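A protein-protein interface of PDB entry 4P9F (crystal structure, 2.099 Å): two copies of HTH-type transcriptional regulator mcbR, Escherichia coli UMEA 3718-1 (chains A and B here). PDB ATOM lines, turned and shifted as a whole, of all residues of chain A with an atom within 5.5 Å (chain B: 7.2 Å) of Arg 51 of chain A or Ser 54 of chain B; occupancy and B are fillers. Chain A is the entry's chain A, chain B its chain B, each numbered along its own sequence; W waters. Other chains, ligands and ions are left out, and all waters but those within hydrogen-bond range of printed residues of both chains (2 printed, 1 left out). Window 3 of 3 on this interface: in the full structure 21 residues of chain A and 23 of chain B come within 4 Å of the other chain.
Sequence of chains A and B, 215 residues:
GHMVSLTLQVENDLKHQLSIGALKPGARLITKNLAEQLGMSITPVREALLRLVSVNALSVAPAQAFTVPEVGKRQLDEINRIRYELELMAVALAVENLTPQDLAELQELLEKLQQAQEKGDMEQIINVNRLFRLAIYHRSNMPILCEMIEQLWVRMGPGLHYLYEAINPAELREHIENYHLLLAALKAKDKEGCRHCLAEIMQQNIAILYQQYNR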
ATOM      1  N   SER A   5     -28.411  23.429  -1.567  1.00  0.00           N
ATOM      2  CA  SER A   5     -27.587  22.320  -1.147  1.00  0.00           C
ATOM      3  C   SER A   5     -28.386  21.046  -1.340  1.00  0.00           C
ATOM      4  O   SER A   5     -29.577  21.010  -1.028  1.00  0.00           O
ATOM      5  CB  SER A   5     -27.183  22.521   0.317  1.00  0.00           C
ATOM      6  OG  SER A   5     -26.930  21.289   0.953  1.00  0.00           O
ATOM      7  N   THR A   7     -27.858  18.337   0.314  1.00  0.00           N
ATOM      8  CA  THR A   7     -28.122  17.870   1.666  1.00  0.00           C
ATOM      9  C   THR A   7     -29.336  18.575   2.295  1.00  0.00           C
ATOM     10  O   THR A   7     -30.189  17.931   2.884  1.00  0.00           O
ATOM     11  CB  THR A   7     -26.905  18.119   2.553  1.00  0.00           C
ATOM     12  OG1 THR A   7     -25.757  17.550   1.924  1.00  0.00           O
ATOM     13  CG2 THR A   7     -27.116  17.517   3.984  1.00  0.00           C
ATOM     14  N   LEU A   8     -29.425  19.891   2.114  1.00  0.00           N
ATOM     15  CA  LEU A   8     -30.542  20.657   2.683  1.00  0.00           C
ATOM     16  C   LEU A   8     -31.858  20.242   2.035  1.00  0.00           C
ATOM     17  O   LEU A   8     -32.881  20.158   2.704  1.00  0.00           O
ATOM     18  CB  LEU A   8     -30.334  22.166   2.490  1.00  0.00           C
ATOM     19  CG  LEU A   8     -31.463  23.099   2.990  1.00  0.00           C
ATOM     20  CD1 LEU A   8     -31.731  22.855   4.490  1.00  0.00           C
ATOM     21  CD2 LEU A   8     -31.096  24.571   2.727  1.00  0.00           C
ATOM     22  N   GLU A  11     -32.932  17.007   3.462  1.00  0.00           N
ATOM     23  CA  GLU A  11     -33.334  17.226   4.836  1.00  0.00           C
ATOM     24  C   GLU A  11     -34.730  17.863   4.952  1.00  0.00           C
ATOM     25  O   GLU A  11     -35.563  17.414   5.743  1.00  0.00           O
ATOM     26  CB  GLU A  11     -32.340  18.131   5.550  1.00  0.00           C
ATOM     27  CG  GLU A  11     -32.702  18.274   7.022  1.00  0.00           C
ATOM     28  CD  GLU A  11     -31.875  19.316   7.732  1.00  0.00           C
ATOM     29  OE1 GLU A  11     -31.138  20.070   7.046  1.00  0.00           O
ATOM     30  OE2 GLU A  11     -31.953  19.356   8.979  1.00  0.00           O
ATOM     31  N   ARG A  46     -27.119  10.573   3.555  1.00  0.00           N
ATOM     32  CA  ARG A  46     -26.681  10.228   4.910  1.00  0.00           C
ATOM     33  C   ARG A  46     -26.559  11.464   5.817  1.00  0.00           C
ATOM     34  O   ARG A  46     -26.977  11.426   6.980  1.00  0.00           O
ATOM     35  CB  ARG A  46     -25.340   9.487   4.874  1.00  0.00           C
ATOM     36  CG  ARG A  46     -24.895   8.998   6.268  1.00  0.00           C
ATOM     37  CD  ARG A  46     -23.461   8.448   6.277  1.00  0.00           C
ATOM     38  NE  ARG A  46     -22.500   9.497   5.953  1.00  0.00           N
ATOM     39  CZ  ARG A  46     -21.814   9.562   4.814  1.00  0.00           C
ATOM     40  NH1 ARG A  46     -21.946   8.611   3.896  1.00  0.00           N
ATOM     41  NH2 ARG A  46     -20.978  10.570   4.602  1.00  0.00           N
ATOM     42  N   GLU A  47     -26.012  12.566   5.295  1.00  0.00           N
ATOM     43  CA  GLU A  47     -25.875  13.768   6.121  1.00  0.00           C
ATOM     44  C   GLU A  47     -27.224  14.339   6.551  1.00  0.00           C
ATOM     45  O   GLU A  47     -27.380  14.820   7.687  1.00  0.00           O
ATOM     46  CB  GLU A  47     -25.085  14.873   5.400  1.00  0.00           C
ATOM     47  CG  GLU A  47     -23.626  14.556   5.182  1.00  0.00           C
ATOM     48  CD  GLU A  47     -22.871  15.698   4.500  1.00  0.00           C
ATOM     49  OE1 GLU A  47     -23.516  16.640   3.986  1.00  0.00           O
ATOM     50  OE2 GLU A  47     -21.626  15.644   4.472  1.00  0.00           O
ATOM     51  N   ALA A  48     -28.188  14.313   5.642  1.00  0.00           N
ATOM     52  CA  ALA A  48     -29.520  14.837   5.940  1.00  0.00           C
ATOM     53  C   ALA A  48     -30.156  14.017   7.053  1.00  0.00           C
ATOM     54  O   ALA A  48     -30.715  14.564   8.004  1.00  0.00           O
ATOM     55  CB  ALA A  48     -30.401  14.821   4.676  1.00  0.00           C
ATOM     56  N   LEU A  49     -30.028  12.697   6.952  1.00  0.00           N
ATOM     57  CA  LEU A  49     -30.565  11.813   7.974  1.00  0.00           C
ATOM     58  C   LEU A  49     -29.888  12.061   9.332  1.00  0.00           C
ATOM     59  O   LEU A  49     -30.560  12.098  10.360  1.00  0.00           O
ATOM     60  CB  LEU A  49     -30.403  10.354   7.530  1.00  0.00           C
ATOM     61  CG  LEU A  49     -31.267   9.941   6.333  1.00  0.00           C
ATOM     62  CD1 LEU A  49     -30.686   8.694   5.647  1.00  0.00           C
ATOM     63  CD2 LEU A  49     -32.692   9.645   6.791  1.00  0.00           C
ATOM     64  N   LEU A  50     -28.570  12.254   9.325  1.00  0.00           N
ATOM     65  CA  LEU A  50     -27.810  12.513  10.556  1.00  0.00           C
ATOM     66  C   LEU A  50     -28.164  13.859  11.156  1.00  0.00           C
ATOM     67  O   LEU A  50     -28.152  14.007  12.379  1.00  0.00           O
ATOM     68  CB  LEU A  50     -26.304  12.416  10.302  1.00  0.00           C
ATOM     69  CG  LEU A  50     -25.837  10.972  10.103  1.00  0.00           C
ATOM     70  CD1 LEU A  50     -24.378  10.902   9.654  1.00  0.00           C
ATOM     71  CD2 LEU A  50     -26.051  10.189  11.397  1.00  0.00           C
ATOM     72  N   ARG A  51     -28.493  14.834  10.306  1.00  0.00           N
ATOM     73  CA  ARG A  51     -28.978  16.123  10.806  1.00  0.00           C
ATOM     74  C   ARG A  51     -30.272  15.930  11.607  1.00  0.00           C
ATOM     75  O   ARG A  51     -30.477  16.570  12.635  1.00  0.00           O
ATOM     76  CB  ARG A  51     -29.246  17.081   9.641  1.00  0.00           C
ATOM     77  CG  ARG A  51     -27.993  17.659   8.971  1.00  0.00           C
ATOM     78  CD  ARG A  51     -28.397  18.651   7.863  1.00  0.00           C
ATOM     79  NE  ARG A  51     -27.219  19.219   7.208  1.00  0.00           N
ATOM     80  CZ  ARG A  51     -27.260  20.175   6.293  1.00  0.00           C
ATOM     81  NH1 ARG A  51     -28.438  20.661   5.898  1.00  0.00           N
ATOM     82  NH2 ARG A  51     -26.126  20.634   5.782  1.00  0.00           N
ATOM     83  N   LEU A  52     -31.138  15.038  11.133  1.00  0.00           N
ATOM     84  CA  LEU A  52     -32.382  14.754  11.830  1.00  0.00           C
ATOM     85  C   LEU A  52     -32.129  13.967  13.124  1.00  0.00           C
ATOM     86  O   LEU A  52     -32.780  14.207  14.149  1.00  0.00           O
ATOM     87  CB  LEU A  52     -33.333  14.012  10.892  1.00  0.00           C
ATOM     88  CG  LEU A  52     -33.849  14.891   9.742  1.00  0.00           C
ATOM     89  CD1 LEU A  52     -34.535  14.063   8.665  1.00  0.00           C
ATOM     90  CD2 LEU A  52     -34.828  15.931  10.283  1.00  0.00           C
ATOM     91  N   VAL A  53     -31.158  13.055  13.089  1.00  0.00           N
ATOM     92  CA  VAL A  53     -30.755  12.338  14.292  1.00  0.00           C
ATOM     93  C   VAL A  53     -30.281  13.330  15.356  1.00  0.00           C
ATOM     94  O   VAL A  53     -30.626  13.199  16.518  1.00  0.00           O
ATOM     95  CB  VAL A  53     -29.657  11.295  14.002  1.00  0.00           C
ATOM     96  CG1 VAL A  53     -28.965  10.809  15.307  1.00  0.00           C
ATOM     97  CG2 VAL A  53     -30.241  10.137  13.199  1.00  0.00           C
ATOM     98  N   SER A  54     -29.509  14.333  14.948  1.00  0.00           N
ATOM     99  CA  SER A  54     -28.923  15.276  15.903  1.00  0.00           C
ATOM    100  C   SER A  54     -29.982  16.110  16.644  1.00  0.00           C
ATOM    101  O   SER A  54     -29.712  16.616  17.735  1.00  0.00           O
ATOM    102  CB  SER A  54     -27.919  16.202  15.206  1.00  0.00           C
ATOM    103  OG  SER A  54     -28.586  17.135  14.382  1.00  0.00           O
ATOM    104  N   VAL A  55     -31.155  16.308  16.047  1.00  0.00           N
ATOM    105  CA  VAL A  55     -32.239  16.981  16.768  1.00  0.00           C
ATOM    106  C   VAL A  55     -33.291  15.977  17.272  1.00  0.00           C
ATOM    107  O   VAL A  55     -34.397  16.368  17.661  1.00  0.00           O
ATOM    108  CB  VAL A  55     -32.914  18.095  15.909  1.00  0.00           C
ATOM    109  CG1 VAL A  55     -31.894  19.169  15.568  1.00  0.00           C
ATOM    110  CG2 VAL A  55     -33.583  17.516  14.654  1.00  0.00           C
ATOM    111  N   LEU B   8     -21.450  12.550  16.494  1.00  0.00           N
ATOM    112  CA  LEU B   8     -22.527  13.075  17.332  1.00  0.00           C
ATOM    113  C   LEU B   8     -21.962  13.575  18.664  1.00  0.00           C
ATOM    114  O   LEU B   8     -22.422  14.574  19.206  1.00  0.00           O
ATOM    115  CB  LEU B   8     -23.605  12.015  17.564  1.00  0.00           C
ATOM    116  CG  LEU B   8     -24.345  11.551  16.302  1.00  0.00           C
ATOM    117  CD1 LEU B   8     -25.252  10.359  16.609  1.00  0.00           C
ATOM    118  CD2 LEU B   8     -25.129  12.707  15.677  1.00  0.00           C
ATOM    119  N   GLU B  11     -20.224  16.932  18.216  1.00  0.00           N
ATOM    120  CA  GLU B  11     -21.255  17.958  18.114  1.00  0.00           C
ATOM    121  C   GLU B  11     -21.714  18.366  19.528  1.00  0.00           C
ATOM    122  O   GLU B  11     -21.857  19.553  19.818  1.00  0.00           O
ATOM    123  CB  GLU B  11     -22.414  17.455  17.251  1.00  0.00           C
ATOM    124  CG  GLU B  11     -23.519  18.466  17.012  1.00  0.00           C
ATOM    125  CD  GLU B  11     -24.650  17.922  16.143  1.00  0.00           C
ATOM    126  OE1 GLU B  11     -24.635  16.719  15.801  1.00  0.00           O
ATOM    127  OE2 GLU B  11     -25.556  18.711  15.804  1.00  0.00           O
ATOM    128  N   GLU B  47     -17.848  16.978   9.824  1.00  0.00           N
ATOM    129  CA  GLU B  47     -19.248  16.607   9.671  1.00  0.00           C
ATOM    130  C   GLU B  47     -20.119  17.222  10.776  1.00  0.00           C
ATOM    131  O   GLU B  47     -21.240  17.671  10.519  1.00  0.00           O
ATOM    132  CB  GLU B  47     -19.390  15.083   9.666  1.00  0.00           C
ATOM    133  CG  GLU B  47     -18.818  14.426   8.423  1.00  0.00           C
ATOM    134  CD  GLU B  47     -18.967  12.919   8.433  1.00  0.00           C
ATOM    135  OE1 GLU B  47     -19.256  12.354   9.510  1.00  0.00           O
ATOM    136  OE2 GLU B  47     -18.808  12.302   7.356  1.00  0.00           O
ATOM    137  N   ALA B  48     -19.593  17.230  11.997  1.00  0.00           N
ATOM    138  CA  ALA B  48     -20.289  17.810  13.141  1.00  0.00           C
ATOM    139  C   ALA B  48     -20.451  19.313  12.975  1.00  0.00           C
ATOM    140  O   ALA B  48     -21.507  19.873  13.260  1.00  0.00           O
ATOM    141  CB  ALA B  48     -19.541  17.493  14.448  1.00  0.00           C
ATOM    142  N   LEU B  49     -19.392  19.968  12.512  1.00  0.00           N
ATOM    143  CA  LEU B  49     -19.416  21.417  12.295  1.00  0.00           C
ATOM    144  C   LEU B  49     -20.455  21.814  11.230  1.00  0.00           C
ATOM    145  O   LEU B  49     -21.155  22.816  11.379  1.00  0.00           O
ATOM    146  CB  LEU B  49     -18.014  21.897  11.896  1.00  0.00           C
ATOM    147  CG  LEU B  49     -16.918  21.756  12.973  1.00  0.00           C
ATOM    148  CD1 LEU B  49     -15.528  21.805  12.372  1.00  0.00           C
ATOM    149  CD2 LEU B  49     -17.049  22.840  14.035  1.00  0.00           C
ATOM    150  N   LEU B  50     -20.542  21.045  10.145  1.00  0.00           N
ATOM    151  CA  LEU B  50     -21.529  21.320   9.092  1.00  0.00           C
ATOM    152  C   LEU B  50     -22.941  21.066   9.600  1.00  0.00           C
ATOM    153  O   LEU B  50     -23.869  21.777   9.228  1.00  0.00           O
ATOM    154  CB  LEU B  50     -21.273  20.451   7.861  1.00  0.00           C
ATOM    155  CG  LEU B  50     -20.076  20.775   6.975  1.00  0.00           C
ATOM    156  CD1 LEU B  50     -19.867  19.677   5.947  1.00  0.00           C
ATOM    157  CD2 LEU B  50     -20.303  22.107   6.280  1.00  0.00           C
ATOM    158  N   ARG B  51     -23.114  20.055  10.448  1.00  0.00           N
ATOM    159  CA  ARG B  51     -24.445  19.854  11.041  1.00  0.00           C
ATOM    160  C   ARG B  51     -24.813  21.017  11.958  1.00  0.00           C
ATOM    161  O   ARG B  51     -25.960  21.458  11.971  1.00  0.00           O
ATOM    162  CB  ARG B  51     -24.548  18.510  11.780  1.00  0.00           C
ATOM    163  CG  ARG B  51     -24.628  17.327  10.806  1.00  0.00           C
ATOM    164  CD  ARG B  51     -25.005  15.997  11.474  1.00  0.00           C
ATOM    165  NE  ARG B  51     -24.340  15.784  12.749  1.00  0.00           N
ATOM    166  CZ  ARG B  51     -23.219  15.092  12.903  1.00  0.00           C
ATOM    167  NH1 ARG B  51     -22.622  14.531  11.857  1.00  0.00           N
ATOM    168  NH2 ARG B  51     -22.699  14.955  14.111  1.00  0.00           N
ATOM    169  N   LEU B  52     -23.837  21.547  12.691  1.00  0.00           N
ATOM    170  CA  LEU B  52     -24.095  22.692  13.561  1.00  0.00           C
ATOM    171  C   LEU B  52     -24.421  23.930  12.737  1.00  0.00           C
ATOM    172  O   LEU B  52     -25.267  24.746  13.132  1.00  0.00           O
ATOM    173  CB  LEU B  52     -22.894  22.959  14.475  1.00  0.00           C
ATOM    174  CG  LEU B  52     -22.705  21.908  15.573  1.00  0.00           C
ATOM    175  CD1 LEU B  52     -21.358  22.062  16.235  1.00  0.00           C
ATOM    176  CD2 LEU B  52     -23.832  22.013  16.599  1.00  0.00           C
ATOM    177  N   VAL B  53     -23.776  24.072  11.585  1.00  0.00           N
ATOM    178  CA  VAL B  53     -24.142  25.161  10.699  1.00  0.00           C
ATOM    179  C   VAL B  53     -25.619  25.037  10.300  1.00  0.00           C
ATOM    180  O   VAL B  53     -26.356  26.029  10.313  1.00  0.00           O
ATOM    181  CB  VAL B  53     -23.255  25.204   9.435  1.00  0.00           C
ATOM    182  CG1 VAL B  53     -23.857  26.151   8.387  1.00  0.00           C
ATOM    183  CG2 VAL B  53     -21.821  25.619   9.791  1.00  0.00           C
ATOM    184  N   SER B  54     -26.060  23.823   9.974  1.00  0.00           N
ATOM    185  CA  SER B  54     -27.437  23.642   9.489  1.00  0.00           C
ATOM    186  C   SER B  54     -28.503  24.009  10.536  1.00  0.00           C
ATOM    187  O   SER B  54     -29.641  24.316  10.177  1.00  0.00           O
ATOM    188  CB  SER B  54     -27.658  22.210   8.997  1.00  0.00           C
ATOM    189  OG  SER B  54     -27.728  21.294  10.079  1.00  0.00           O
ATOM    190  N   VAL B  55     -28.165  23.941  11.826  1.00  0.00           N
ATOM    191  CA  VAL B  55     -29.121  24.376  12.865  1.00  0.00           C
ATOM    192  C   VAL B  55     -28.779  25.785  13.382  1.00  0.00           C
ATOM    193  O   VAL B  55     -29.304  26.228  14.415  1.00  0.00           O
ATOM    194  CB  VAL B  55     -29.171  23.417  14.078  1.00  0.00           C
ATOM    195  CG1 VAL B  55     -29.501  22.008  13.609  1.00  0.00           C
ATOM    196  CG2 VAL B  55     -27.834  23.413  14.847  1.00  0.00           C
ATOM    197  N   ASN B  56     -27.880  26.457  12.667  1.00  0.00           N
ATOM    198  CA  ASN B  56     -27.459  27.823  12.970  1.00  0.00           C
ATOM    199  C   ASN B  56     -26.788  27.964  14.331  1.00  0.00           C
ATOM    200  O   ASN B  56     -26.776  29.044  14.904  1.00  0.00           O
ATOM    201  CB  ASN B  56     -28.649  28.780  12.864  1.00  0.00           C
ATOM    202  CG  ASN B  56     -29.205  28.851  11.449  1.00  0.00           C
ATOM    203  OD1 ASN B  56     -28.453  28.987  10.486  1.00  0.00           O
ATOM    204  ND2 ASN B  56     -30.514  28.701  11.318  1.00  0.00           N
ATOM    205  N   ALA B  57     -26.218  26.875  14.835  1.00  0.00           N
ATOM    206  CA  ALA B  57     -25.417  26.941  16.053  1.00  0.00           C
ATOM    207  C   ALA B  57     -24.038  27.449  15.667  1.00  0.00           C
ATOM    208  O   ALA B  57     -23.326  28.011  16.485  1.00  0.00           O
ATOM    209  CB  ALA B  57     -25.320  25.595  16.722  1.00  0.00           C
ATOM    210  N   LEU B  58     -23.689  27.272  14.394  1.00  0.00           N
ATOM    211  CA  LEU B  58     -22.462  27.843  13.849  1.00  0.00           C
ATOM    212  C   LEU B  58     -22.772  28.517  12.524  1.00  0.00           C
ATOM    213  O   LEU B  58     -23.847  28.320  11.946  1.00  0.00           O
ATOM    214  CB  LEU B  58     -21.383  26.777  13.651  1.00  0.00           C
ATOM    215  CG  LEU B  58     -20.742  26.164  14.898  1.00  0.00           C
ATOM    216  CD1 LEU B  58     -19.768  25.066  14.459  1.00  0.00           C
ATOM    217  CD2 LEU B  58     -20.021  27.245  15.713  1.00  0.00           C
HETATM  218  O   HOH W   1     -31.395  22.985   7.917  1.00  0.00           O
HETATM  219  O   HOH W   2     -30.445  20.808  10.485  1.00  0.00           O
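The guanidinium group (NH2) of Arg 46 of chain A is in salt-bridge range of the side-chain carboxylate (OE2) of Glu 47 of chain B (3.9 Å).
OG of Ser 54 of chain B lies within hydrogen-bond range of O of Arg 51 of chain B (2.6 Å).
The backbone carbonyl oxygen of Arg 51 of chain A is in hydrogen-bond range of the side-chain hydroxyl of Ser 54 of chain A (2.6 Å).
The side-chain carboxylate (OE1) of Glu 11 of chain A lies within salt-bridge range of the guanidinium group (NH1) of Arg 51 of chain A, at 3.0 Å.
The side-chain carboxylate of Glu 11 of chain B lies within salt-bridge range of the guanidinium group of Arg 51 of chain B, at 3.1 Å.
Leu 50 of chain A touches Arg 51 of chain B (C to CD, 3.8 Å).
Arg 51 of chain A touches Arg 51 of chain B.
Arg 51 of chain A touches Ser 54 of chain B.
Val 53 of chain A touches Leu 8 of chain B (CG1 to CD1, 3.96 Å).
Ser 54 of chain A touches Glu 11 of chain B.
Leu 8 of chain A touches none of the printed residues of chain B.
Of chain B, only Arg 51 and Ser 54 come within 4 Å of Arg 51 of chain A.
Printed residues of chain A within 4 Å of Glu 11 of chain B: Ser 54.
Printed residues of chain A within 4 Å of Arg 51 of chain B: Leu 50 and Arg 51.
Printed residues of chain A within 4 Å of Ser 54 of chain B: Arg 51 (3.4 Å).
The nearest residue of chain B that does not touch Arg 51 of chain A is Leu 50 of chain B (4.3 Å).
The nearest residue of chain A that does not touch Ser 54 of chain B is Glu 11 of chain A (4.5 Å).
The nearest printed residue of chain B that does not touch Val 53 of chain A is Glu 11 of chain B (6.6 Å).
Leu 50 of chain A touches Arg 51 of chain B, but with the chains exchanged Arg 51 of chain A does not touch Leu 50 of chain B (4.3 Å).
Arg 51 of chain A touches Ser 54 of chain B, but with the chains exchanged Ser 54 of chain A does not touch Arg 51 of chain B (4.4 Å).
Val 53 of chain A touches Leu 8 of chain B, but with the chains exchanged Leu 8 of chain A does not touch Val 53 of chain B (8.5 Å).
Ser 54 of chain A touches Glu 11 of chain B, but with the chains exchanged Glu 11 of chain A does not touch Ser 54 of chain B (4.5 Å).
Positions printed for both chains: 8, 11, 47, 48, 49, 50, 51, 52, 53, 54 and 55.
Of the 6 pairs that touch across the chains among the printed residues, 1 has its exchanged pair printed and touching as well.
Water W2 bridges OE2 of Glu 11 of chain A (2.6 Å) and OG of Ser 54 of chain B (2.8 Å).
Water W1 bridges OE1 of Glu 11 of chain A and O of Ser 54 of chain B.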
